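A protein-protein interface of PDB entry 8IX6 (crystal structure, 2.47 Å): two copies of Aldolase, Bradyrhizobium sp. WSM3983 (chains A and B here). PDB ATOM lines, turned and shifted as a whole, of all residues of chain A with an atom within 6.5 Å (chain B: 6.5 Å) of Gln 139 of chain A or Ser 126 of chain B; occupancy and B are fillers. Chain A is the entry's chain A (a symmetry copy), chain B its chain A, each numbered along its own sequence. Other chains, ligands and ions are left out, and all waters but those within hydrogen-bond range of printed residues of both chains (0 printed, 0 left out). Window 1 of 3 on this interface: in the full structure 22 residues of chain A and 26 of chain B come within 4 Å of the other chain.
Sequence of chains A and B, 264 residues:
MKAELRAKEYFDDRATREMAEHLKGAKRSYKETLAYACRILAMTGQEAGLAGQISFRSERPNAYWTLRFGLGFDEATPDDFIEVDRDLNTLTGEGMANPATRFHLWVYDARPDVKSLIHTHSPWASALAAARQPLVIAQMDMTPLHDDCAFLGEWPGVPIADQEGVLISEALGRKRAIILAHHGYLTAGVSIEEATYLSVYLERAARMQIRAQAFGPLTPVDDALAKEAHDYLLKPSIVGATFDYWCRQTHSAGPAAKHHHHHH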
ATOM      1  N   VAL A 136       0.851  15.378 -10.868  1.00  0.00           N
ATOM      2  CA  VAL A 136       1.274  14.031 -10.498  1.00  0.00           C
ATOM      3  C   VAL A 136       1.391  14.000  -8.981  1.00  0.00           C
ATOM      4  O   VAL A 136       2.282  14.635  -8.402  1.00  0.00           O
ATOM      5  CB  VAL A 136       2.596  13.634 -11.171  1.00  0.00           C
ATOM      6  CG1 VAL A 136       3.138  12.350 -10.553  1.00  0.00           C
ATOM      7  CG2 VAL A 136       2.402  13.462 -12.672  1.00  0.00           C
ATOM      8  N   ILE A 137       0.492  13.263  -8.334  1.00  0.00           N
ATOM      9  CA  ILE A 137       0.425  13.230  -6.875  1.00  0.00           C
ATOM     10  C   ILE A 137       1.630  12.450  -6.355  1.00  0.00           C
ATOM     11  O   ILE A 137       1.676  11.222  -6.456  1.00  0.00           O
ATOM     12  CB  ILE A 137      -0.888  12.609  -6.387  1.00  0.00           C
ATOM     13  CG1 ILE A 137      -2.087  13.245  -7.101  1.00  0.00           C
ATOM     14  CG2 ILE A 137      -1.012  12.768  -4.883  1.00  0.00           C
ATOM     15  CD1 ILE A 137      -2.107  14.762  -7.040  1.00  0.00           C
ATOM     16  N   ALA A 138       2.602  13.159  -5.778  1.00  0.00           N
ATOM     17  CA  ALA A 138       3.828  12.533  -5.302  1.00  0.00           C
ATOM     18  C   ALA A 138       4.198  12.941  -3.881  1.00  0.00           C
ATOM     19  O   ALA A 138       5.264  12.543  -3.397  1.00  0.00           O
ATOM     20  CB  ALA A 138       4.993  12.850  -6.243  1.00  0.00           C
ATOM     21  N   GLN A 139       3.363  13.725  -3.205  1.00  0.00           N
ATOM     22  CA  GLN A 139       3.662  14.157  -1.848  1.00  0.00           C
ATOM     23  C   GLN A 139       2.350  14.334  -1.096  1.00  0.00           C
ATOM     24  O   GLN A 139       1.290  14.521  -1.697  1.00  0.00           O
ATOM     25  CB  GLN A 139       4.497  15.445  -1.848  1.00  0.00           C
ATOM     26  CG  GLN A 139       5.079  15.832  -0.498  1.00  0.00           C
ATOM     27  CD  GLN A 139       4.224  16.846   0.228  1.00  0.00           C
ATOM     28  OE1 GLN A 139       3.308  17.428  -0.352  1.00  0.00           O
ATOM     29  NE2 GLN A 139       4.524  17.072   1.500  1.00  0.00           N
ATOM     30  N   MET A 140       2.438  14.262   0.235  1.00  0.00           N
ATOM     31  CA  MET A 140       1.241  14.205   1.074  1.00  0.00           C
ATOM     32  C   MET A 140       0.322  15.398   0.836  1.00  0.00           C
ATOM     33  O   MET A 140      -0.895  15.238   0.685  1.00  0.00           O
ATOM     34  CB  MET A 140       1.647  14.125   2.545  1.00  0.00           C
ATOM     35  CG  MET A 140       0.594  14.634   3.515  1.00  0.00           C
ATOM     36  SD  MET A 140      -0.479  13.312   4.109  1.00  0.00           S
ATOM     37  CE  MET A 140       0.730  12.194   4.809  1.00  0.00           C
ATOM     38  N   ASP A 141       0.884  16.605   0.804  1.00  0.00           N
ATOM     39  CA  ASP A 141       0.064  17.798   0.629  1.00  0.00           C
ATOM     40  C   ASP A 141      -0.529  17.910  -0.771  1.00  0.00           C
ATOM     41  O   ASP A 141      -1.307  18.838  -1.016  1.00  0.00           O
ATOM     42  CB  ASP A 141       0.886  19.048   0.953  1.00  0.00           C
ATOM     43  CG  ASP A 141       1.208  19.170   2.434  1.00  0.00           C
ATOM     44  OD1 ASP A 141       0.290  18.999   3.265  1.00  0.00           O
ATOM     45  OD2 ASP A 141       2.379  19.442   2.768  1.00  0.00           O
ATOM     46  N   MET A 142      -0.186  17.000  -1.684  1.00  0.00           N
ATOM     47  CA  MET A 142      -0.775  16.969  -3.016  1.00  0.00           C
ATOM     48  C   MET A 142      -2.018  16.093  -3.082  1.00  0.00           C
ATOM     49  O   MET A 142      -2.763  16.173  -4.064  1.00  0.00           O
ATOM     50  CB  MET A 142       0.247  16.461  -4.040  1.00  0.00           C
ATOM     51  CG  MET A 142       1.295  17.481  -4.431  1.00  0.00           C
ATOM     52  SD  MET A 142       2.688  16.770  -5.327  1.00  0.00           S
ATOM     53  CE  MET A 142       2.424  17.489  -6.947  1.00  0.00           C
ATOM     54  N   THR A 143      -2.251  15.269  -2.062  1.00  0.00           N
ATOM     55  CA  THR A 143      -3.352  14.314  -2.107  1.00  0.00           C
ATOM     56  C   THR A 143      -4.748  14.935  -2.173  1.00  0.00           C
ATOM     57  O   THR A 143      -5.639  14.275  -2.735  1.00  0.00           O
ATOM     58  CB  THR A 143      -3.251  13.365  -0.903  1.00  0.00           C
ATOM     59  OG1 THR A 143      -3.263  14.120   0.315  1.00  0.00           O
ATOM     60  CG2 THR A 143      -1.969  12.549  -0.980  1.00  0.00           C
ATOM     61  N   PRO A 144      -5.027  16.152  -1.631  1.00  0.00           N
ATOM     62  CA  PRO A 144      -6.372  16.728  -1.798  1.00  0.00           C
ATOM     63  C   PRO A 144      -6.846  16.794  -3.243  1.00  0.00           C
ATOM     64  O   PRO A 144      -8.048  16.919  -3.503  1.00  0.00           O
ATOM     65  CB  PRO A 144      -6.219  18.133  -1.206  1.00  0.00           C
ATOM     66  CG  PRO A 144      -5.209  17.967  -0.151  1.00  0.00           C
ATOM     67  CD  PRO A 144      -4.238  16.932  -0.656  1.00  0.00           C
ATOM     68  N   MET A 208       5.744  22.306  -6.095  1.00  0.00           N
ATOM     69  CA  MET A 208       6.447  21.107  -5.654  1.00  0.00           C
ATOM     70  C   MET A 208       6.767  20.194  -6.830  1.00  0.00           C
ATOM     71  O   MET A 208       7.886  19.679  -6.948  1.00  0.00           O
ATOM     72  CB  MET A 208       5.601  20.371  -4.616  1.00  0.00           C
ATOM     73  CG  MET A 208       6.389  19.474  -3.693  1.00  0.00           C
ATOM     74  SD  MET A 208       5.322  18.794  -2.417  1.00  0.00           S
ATOM     75  CE  MET A 208       4.597  20.290  -1.743  1.00  0.00           C
ATOM     76  N   ALA A 212      10.525  19.269  -8.145  1.00  0.00           N
ATOM     77  CA  ALA A 212      10.917  17.864  -8.124  1.00  0.00           C
ATOM     78  C   ALA A 212      11.259  17.337  -9.510  1.00  0.00           C
ATOM     79  O   ALA A 212      11.951  16.319  -9.620  1.00  0.00           O
ATOM     80  CB  ALA A 212       9.805  17.016  -7.504  1.00  0.00           C
ATOM     81  N   VAL A 221       2.521   8.482  -5.854  1.00  0.00           N
ATOM     82  CA  VAL A 221       2.287   7.611  -4.713  1.00  0.00           C
ATOM     83  C   VAL A 221       1.195   6.599  -5.047  1.00  0.00           C
ATOM     84  O   VAL A 221       0.463   6.721  -6.036  1.00  0.00           O
ATOM     85  CB  VAL A 221       1.929   8.432  -3.462  1.00  0.00           C
ATOM     86  CG1 VAL A 221       3.013   9.457  -3.184  1.00  0.00           C
ATOM     87  CG2 VAL A 221       0.573   9.100  -3.634  1.00  0.00           C
ATOM     88  N   ALA B  48       3.524  24.916   6.023  1.00  0.00           N
ATOM     89  CA  ALA B  48       2.630  24.563   4.918  1.00  0.00           C
ATOM     90  C   ALA B  48       1.279  24.207   5.540  1.00  0.00           C
ATOM     91  O   ALA B  48       0.929  23.036   5.706  1.00  0.00           O
ATOM     92  CB  ALA B  48       3.191  23.417   4.078  1.00  0.00           C
ATOM     93  N   THR B 120       8.023  19.254   9.657  1.00  0.00           N
ATOM     94  CA  THR B 120       7.283  20.180   8.812  1.00  0.00           C
ATOM     95  C   THR B 120       7.282  19.670   7.380  1.00  0.00           C
ATOM     96  O   THR B 120       8.067  18.795   7.006  1.00  0.00           O
ATOM     97  CB  THR B 120       7.871  21.601   8.836  1.00  0.00           C
ATOM     98  OG1 THR B 120       9.001  21.666   7.959  1.00  0.00           O
ATOM     99  CG2 THR B 120       8.309  21.990  10.235  1.00  0.00           C
ATOM    100  N   HIS B 121       6.383  20.237   6.577  1.00  0.00           N
ATOM    101  CA  HIS B 121       6.355  19.966   5.145  1.00  0.00           C
ATOM    102  C   HIS B 121       6.891  21.176   4.390  1.00  0.00           C
ATOM    103  O   HIS B 121       6.201  21.731   3.529  1.00  0.00           O
ATOM    104  CB  HIS B 121       4.937  19.631   4.671  1.00  0.00           C
ATOM    105  CG  HIS B 121       4.269  18.536   5.446  1.00  0.00           C
ATOM    106  ND1 HIS B 121       3.004  18.081   5.143  1.00  0.00           N
ATOM    107  CD2 HIS B 121       4.687  17.801   6.505  1.00  0.00           C
ATOM    108  CE1 HIS B 121       2.671  17.118   5.983  1.00  0.00           C
ATOM    109  NE2 HIS B 121       3.675  16.929   6.820  1.00  0.00           N
ATOM    110  N   SER B 122       8.117  21.588   4.709  1.00  0.00           N
ATOM    111  CA  SER B 122       8.697  22.776   4.101  1.00  0.00           C
ATOM    112  C   SER B 122       8.833  22.589   2.589  1.00  0.00           C
ATOM    113  O   SER B 122       8.966  21.460   2.106  1.00  0.00           O
ATOM    114  CB  SER B 122      10.058  23.074   4.728  1.00  0.00           C
ATOM    115  OG  SER B 122      10.731  21.878   5.074  1.00  0.00           O
ATOM    116  N   PRO B 123       8.807  23.683   1.816  1.00  0.00           N
ATOM    117  CA  PRO B 123       8.691  23.537   0.350  1.00  0.00           C
ATOM    118  C   PRO B 123       9.824  22.758  -0.299  1.00  0.00           C
ATOM    119  O   PRO B 123       9.564  21.817  -1.062  1.00  0.00           O
ATOM    120  CB  PRO B 123       8.646  24.994  -0.142  1.00  0.00           C
ATOM    121  CG  PRO B 123       8.275  25.807   1.051  1.00  0.00           C
ATOM    122  CD  PRO B 123       8.833  25.096   2.234  1.00  0.00           C
ATOM    123  N   TRP B 124      11.078  23.125  -0.031  1.00  0.00           N
ATOM    124  CA  TRP B 124      12.190  22.486  -0.728  1.00  0.00           C
ATOM    125  C   TRP B 124      12.411  21.062  -0.239  1.00  0.00           C
ATOM    126  O   TRP B 124      12.705  20.164  -1.039  1.00  0.00           O
ATOM    127  CB  TRP B 124      13.460  23.318  -0.563  1.00  0.00           C
ATOM    128  CG  TRP B 124      13.397  24.635  -1.268  1.00  0.00           C
ATOM    129  CD1 TRP B 124      13.069  25.840  -0.721  1.00  0.00           C
ATOM    130  CD2 TRP B 124      13.659  24.883  -2.656  1.00  0.00           C
ATOM    131  NE1 TRP B 124      13.115  26.824  -1.679  1.00  0.00           N
ATOM    132  CE2 TRP B 124      13.474  26.262  -2.876  1.00  0.00           C
ATOM    133  CE3 TRP B 124      14.035  24.072  -3.732  1.00  0.00           C
ATOM    134  CZ2 TRP B 124      13.652  26.849  -4.127  1.00  0.00           C
ATOM    135  CZ3 TRP B 124      14.211  24.658  -4.974  1.00  0.00           C
ATOM    136  CH2 TRP B 124      14.020  26.031  -5.161  1.00  0.00           C
ATOM    137  N   ALA B 125      12.281  20.833   1.070  1.00  0.00           N
ATOM    138  CA  ALA B 125      12.451  19.485   1.601  1.00  0.00           C
ATOM    139  C   ALA B 125      11.342  18.551   1.131  1.00  0.00           C
ATOM    140  O   ALA B 125      11.592  17.361   0.908  1.00  0.00           O
ATOM    141  CB  ALA B 125      12.507  19.525   3.128  1.00  0.00           C
ATOM    142  N   SER B 126      10.120  19.067   0.974  1.00  0.00           N
ATOM    143  CA  SER B 126       9.026  18.237   0.481  1.00  0.00           C
ATOM    144  C   SER B 126       9.194  17.907  -0.996  1.00  0.00           C
ATOM    145  O   SER B 126       8.801  16.820  -1.433  1.00  0.00           O
ATOM    146  CB  SER B 126       7.685  18.929   0.713  1.00  0.00           C
ATOM    147  OG  SER B 126       7.558  19.350   2.057  1.00  0.00           O
ATOM    148  N   ALA B 127       9.756  18.832  -1.777  1.00  0.00           N
ATOM    149  CA  ALA B 127      10.049  18.537  -3.176  1.00  0.00           C
ATOM    150  C   ALA B 127      11.094  17.436  -3.292  1.00  0.00           C
ATOM    151  O   ALA B 127      10.959  16.525  -4.118  1.00  0.00           O
ATOM    152  CB  ALA B 127      10.517  19.803  -3.896  1.00  0.00           C
ATOM    153  N   LEU B 128      12.143  17.501  -2.468  1.00  0.00           N
ATOM    154  CA  LEU B 128      13.125  16.424  -2.419  1.00  0.00           C
ATOM    155  C   LEU B 128      12.476  15.107  -2.016  1.00  0.00           C
ATOM    156  O   LEU B 128      12.782  14.052  -2.586  1.00  0.00           O
ATOM    157  CB  LEU B 128      14.248  16.785  -1.445  1.00  0.00           C
ATOM    158  CG  LEU B 128      15.657  16.274  -1.749  1.00  0.00           C
ATOM    159  CD1 LEU B 128      16.189  16.898  -3.025  1.00  0.00           C
ATOM    160  CD2 LEU B 128      16.594  16.547  -0.580  1.00  0.00           C
ATOM    161  N   ALA B 129      11.571  15.148  -1.034  1.00  0.00           N
ATOM    162  CA  ALA B 129      10.899  13.932  -0.591  1.00  0.00           C
ATOM    163  C   ALA B 129       9.935  13.414  -1.650  1.00  0.00           C
ATOM    164  O   ALA B 129       9.774  12.199  -1.811  1.00  0.00           O
ATOM    165  CB  ALA B 129      10.165  14.191   0.723  1.00  0.00           C
ATOM    166  N   ALA B 130       9.277  14.322  -2.379  1.00  0.00           N
ATOM    167  CA  ALA B 130       8.361  13.901  -3.432  1.00  0.00           C
ATOM    168  C   ALA B 130       9.087  13.166  -4.548  1.00  0.00           C
ATOM    169  O   ALA B 130       8.523  12.252  -5.160  1.00  0.00           O
ATOM    170  CB  ALA B 130       7.611  15.109  -3.994  1.00  0.00           C
ATOM    171  N   ALA B 131      10.334  13.542  -4.828  1.00  0.00           N
ATOM    172  CA  ALA B 131      11.137  12.888  -5.848  1.00  0.00           C
ATOM    173  C   ALA B 131      11.930  11.707  -5.304  1.00  0.00           C
ATOM    174  O   ALA B 131      12.771  11.159  -6.023  1.00  0.00           O
ATOM    175  CB  ALA B 131      12.088  13.897  -6.498  1.00  0.00           C
ATOM    176  N   TRP B 155       6.178   5.626   2.210  1.00  0.00           N
ATOM    177  CA  TRP B 155       5.210   6.610   2.663  1.00  0.00           C
ATOM    178  C   TRP B 155       3.966   5.873   3.131  1.00  0.00           C
ATOM    179  O   TRP B 155       3.242   5.310   2.295  1.00  0.00           O
ATOM    180  CB  TRP B 155       4.862   7.595   1.551  1.00  0.00           C
ATOM    181  CG  TRP B 155       3.759   8.523   1.938  1.00  0.00           C
ATOM    182  CD1 TRP B 155       3.772   9.425   2.960  1.00  0.00           C
ATOM    183  CD2 TRP B 155       2.468   8.627   1.327  1.00  0.00           C
ATOM    184  NE1 TRP B 155       2.574  10.093   3.017  1.00  0.00           N
ATOM    185  CE2 TRP B 155       1.755   9.621   2.026  1.00  0.00           C
ATOM    186  CE3 TRP B 155       1.849   7.980   0.253  1.00  0.00           C
ATOM    187  CZ2 TRP B 155       0.454   9.984   1.686  1.00  0.00           C
ATOM    188  CZ3 TRP B 155       0.557   8.341  -0.081  1.00  0.00           C
ATOM    189  CH2 TRP B 155      -0.126   9.334   0.633  1.00  0.00           C
ATOM    190  N   LEU B 180      11.403  11.982   4.929  1.00  0.00           N
ATOM    191  CA  LEU B 180      10.264  11.084   4.794  1.00  0.00           C
ATOM    192  C   LEU B 180       9.733  11.213   3.373  1.00  0.00           C
ATOM    193  O   LEU B 180       9.155  12.244   3.012  1.00  0.00           O
ATOM    194  CB  LEU B 180       9.193  11.416   5.830  1.00  0.00           C
ATOM    195  CG  LEU B 180       9.733  11.600   7.251  1.00  0.00           C
ATOM    196  CD1 LEU B 180       8.785  12.445   8.088  1.00  0.00           C
ATOM    197  CD2 LEU B 180       9.985  10.252   7.918  1.00  0.00           C
ATOM    198  N   ALA B 181       9.942  10.170   2.567  1.00  0.00           N
ATOM    199  CA  ALA B 181       9.564  10.206   1.161  1.00  0.00           C
ATOM    200  C   ALA B 181       8.084  10.527   1.002  1.00  0.00           C
ATOM    201  O   ALA B 181       7.243  10.059   1.775  1.00  0.00           O
ATOM    202  CB  ALA B 181       9.886   8.866   0.496  1.00  0.00           C
ATOM    203  N   HIS B 182       7.776  11.344  -0.007  1.00  0.00           N
ATOM    204  CA  HIS B 182       6.418  11.793  -0.310  1.00  0.00           C
ATOM    205  C   HIS B 182       5.767  12.517   0.863  1.00  0.00           C
ATOM    206  O   HIS B 182       4.536  12.554   0.967  1.00  0.00           O
ATOM    207  CB  HIS B 182       5.527  10.625  -0.754  1.00  0.00           C
ATOM    208  CG  HIS B 182       6.158   9.733  -1.778  1.00  0.00           C
ATOM    209  ND1 HIS B 182       6.363  10.127  -3.082  1.00  0.00           N
ATOM    210  CD2 HIS B 182       6.619   8.464  -1.690  1.00  0.00           C
ATOM    211  CE1 HIS B 182       6.930   9.140  -3.754  1.00  0.00           C
ATOM    212  NE2 HIS B 182       7.094   8.118  -2.932  1.00  0.00           N
ATOM    213  N   HIS B 183       6.562  13.107   1.754  1.00  0.00           N
ATOM    214  CA  HIS B 183       6.014  13.674   2.978  1.00  0.00           C
ATOM    215  C   HIS B 183       6.747  14.948   3.372  1.00  0.00           C
ATOM    216  O   HIS B 183       6.270  16.058   3.110  1.00  0.00           O
ATOM    217  CB  HIS B 183       6.086  12.645   4.107  1.00  0.00           C
ATOM    218  CG  HIS B 183       5.292  13.017   5.318  1.00  0.00           C
ATOM    219  ND1 HIS B 183       5.357  12.304   6.497  1.00  0.00           N
ATOM    220  CD2 HIS B 183       4.413  14.023   5.536  1.00  0.00           C
ATOM    221  CE1 HIS B 183       4.553  12.856   7.387  1.00  0.00           C
ATOM    222  NE2 HIS B 183       3.969  13.901   6.830  1.00  0.00           N
ATOM    223  N   GLY B 184       7.906  14.795   4.004  1.00  0.00           N
ATOM    224  CA  GLY B 184       8.701  15.922   4.443  1.00  0.00           C
ATOM    225  C   GLY B 184       9.956  15.469   5.158  1.00  0.00           C
ATOM    226  O   GLY B 184      10.676  14.600   4.660  1.00  0.00           O
ATOM    227  N   TYR B 185      10.222  16.039   6.330  1.00  0.00           N
ATOM    228  CA  TYR B 185      11.391  15.671   7.114  1.00  0.00           C
ATOM    229  C   TYR B 185      11.037  15.693   8.593  1.00  0.00           C
ATOM    230  O   TYR B 185       9.950  16.118   8.995  1.00  0.00           O
ATOM    231  CB  TYR B 185      12.575  16.610   6.840  1.00  0.00           C
ATOM    232  CG  TYR B 185      12.438  17.959   7.509  1.00  0.00           C
ATOM    233  CD1 TYR B 185      11.747  18.990   6.890  1.00  0.00           C
ATOM    234  CD2 TYR B 185      13.001  18.207   8.757  1.00  0.00           C
ATOM    235  CE1 TYR B 185      11.612  20.222   7.493  1.00  0.00           C
ATOM    236  CE2 TYR B 185      12.868  19.441   9.370  1.00  0.00           C
ATOM    237  CZ  TYR B 185      12.172  20.444   8.729  1.00  0.00           C
ATOM    238  OH  TYR B 185      12.030  21.677   9.320  1.00  0.00           O
ATOM    239  N   GLU B 203      16.427  22.278   5.267  1.00  0.00           N
ATOM    240  CA  GLU B 203      15.609  22.895   4.229  1.00  0.00           C
ATOM    241  C   GLU B 203      16.464  23.661   3.228  1.00  0.00           C
ATOM    242  O   GLU B 203      16.211  23.610   2.018  1.00  0.00           O
ATOM    243  CB  GLU B 203      14.566  23.815   4.864  1.00  0.00           C
ATOM    244  CG  GLU B 203      13.862  24.735   3.881  1.00  0.00           C
ATOM    245  CD  GLU B 203      12.827  24.021   3.026  1.00  0.00           C
ATOM    246  OE1 GLU B 203      12.750  22.774   3.072  1.00  0.00           O
ATOM    247  OE2 GLU B 203      12.085  24.715   2.300  1.00  0.00           O
ATOM    248  N   ALA B 206      18.229  21.210   1.084  1.00  0.00           N
ATOM    249  CA  ALA B 206      17.367  20.705   0.021  1.00  0.00           C
ATOM    250  C   ALA B 206      17.272  21.705  -1.124  1.00  0.00           C
ATOM    251  O   ALA B 206      17.366  21.333  -2.300  1.00  0.00           O
ATOM    252  CB  ALA B 206      15.980  20.386   0.581  1.00  0.00           C
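Gln 139 of chain A touches just these residues of chain B: Ser 126, Ala 130, His 182 and His 183.
Thr 143 of chain A touches none of the printed residues of chain B.
Ala 48 of chain B touches none of the printed residues of chain A.
Ser 126 of chain B touches two residues of chain A.
Of the printed residues of chain A, Ala 130 of chain B touches Ala 138 (3.4 Å) and Gln 139 (3.8 Å).
Of the printed residues of chain A, Trp 155 of chain B touches Met 140 (3.3 Å) and Val 221 (3.6 Å).
Of the printed residues of chain A, His 183 of chain B touches Gln 139.
The nearest residue of chain B that does not touch Gln 139 of chain A is His 121 of chain B (4.1 Å).
O of Ala 138 of chain A touches CA of Ala 130 of chain B, at 3.4 Å.
Gln 139 of chain A touches Ser 126 of chain B (NE2 to CB, 3.7 Å).
Gln 139 of chain A touches Ala 130 of chain B (CB to CB, 3.8 Å).
Gln 139 of chain A touches His 182 of chain B.
Met 140 of chain A touches Trp 155 of chain B (CE to NE1, 3.3 Å).
SD of Met 208 of chain A touches CB of Ser 126 of chain B, 3.9 Å away.
CB of Ala 212 of chain A touches O of Ala 127 of chain B, 3.6 Å away.
Ala 212 of chain A touches Ala 131 of chain B (O to CB, 3.95 Å).
Trp 155 of chain B touches Val 221 of chain A.
Val 221 of chain A touches His 182 of chain B (CG1 to ND1, 3.4 Å).
Of the 12 printed residues of chain A, 7 touch a printed residue of chain B.
Hydrophobic or aromatic side chains of chain A within 4 Å of the printed part of chain B: Ala 138, Met 140, Met 208, Ala 212 and Val 221.
Hydrophobic or aromatic side chains of chain B within 4 Å of the printed part of chain A: His 121, Ala 130, Ala 131, Trp 155 and His 182.
Among the printed residues, 15 pairs touch across the chains.
Among the printed residues, no Asp or Glu carboxylate lies within 4 Å of a Lys or Arg side-chain nitrogen of the other chain.
No position is printed for both chains.
Of the 15 pairs that touch across the chains among the printed residues, none has its exchanged pair printed and touching as well.
A ring nitrogen (ND1) of His 121 of chain B lies within hydrogen-bond range of the side-chain carboxylate (OD2) of Asp 141 of chain A (2.8 Å).
The backbone carbonyl oxygen of Ala 138 of chain A is in hydrogen-bond range of a ring nitrogen (ND1) of His 182 of chain B, at 2.7 Å.
The backbone NH (N) of Met 140 of chain A is in hydrogen-bond range of the backbone carbonyl oxygen (O) of His 182 of chain B, at 2.8 Å.
The backbone carbonyl oxygen of His 183 of chain B sits at hydrogen-bond distance from the side-chain amide nitrogen of Gln 139 of chain A.
The backbone carbonyl oxygen of His 121 of chain B sits close to the side-chain hydroxyl of Ser 126 of chain B, at 3.1 Å.
OG of Ser 126 of chain B lies within hydrogen-bond range of O of Ser 122 of chain B, 2.5 Å away.
The backbone NH (N) of Val 221 of chain A is in hydrogen-bond range of the backbone carbonyl oxygen (O) of Ile 137 of chain A (2.9 Å).
OE1 of Gln 139 of chain A lies within hydrogen-bond range of N of Asp 141 of chain A (2.8 Å).
The backbone NH (N) of Gln 139 of chain A is in hydrogen-bond range of the side-chain sulfur (SD) of Met 142 of chain A, 3.8 Å away.
The side-chain amide oxygen (OE1) of Gln 139 of chain A lies close to the side-chain sulfur (SD) of Met 208 of chain A.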
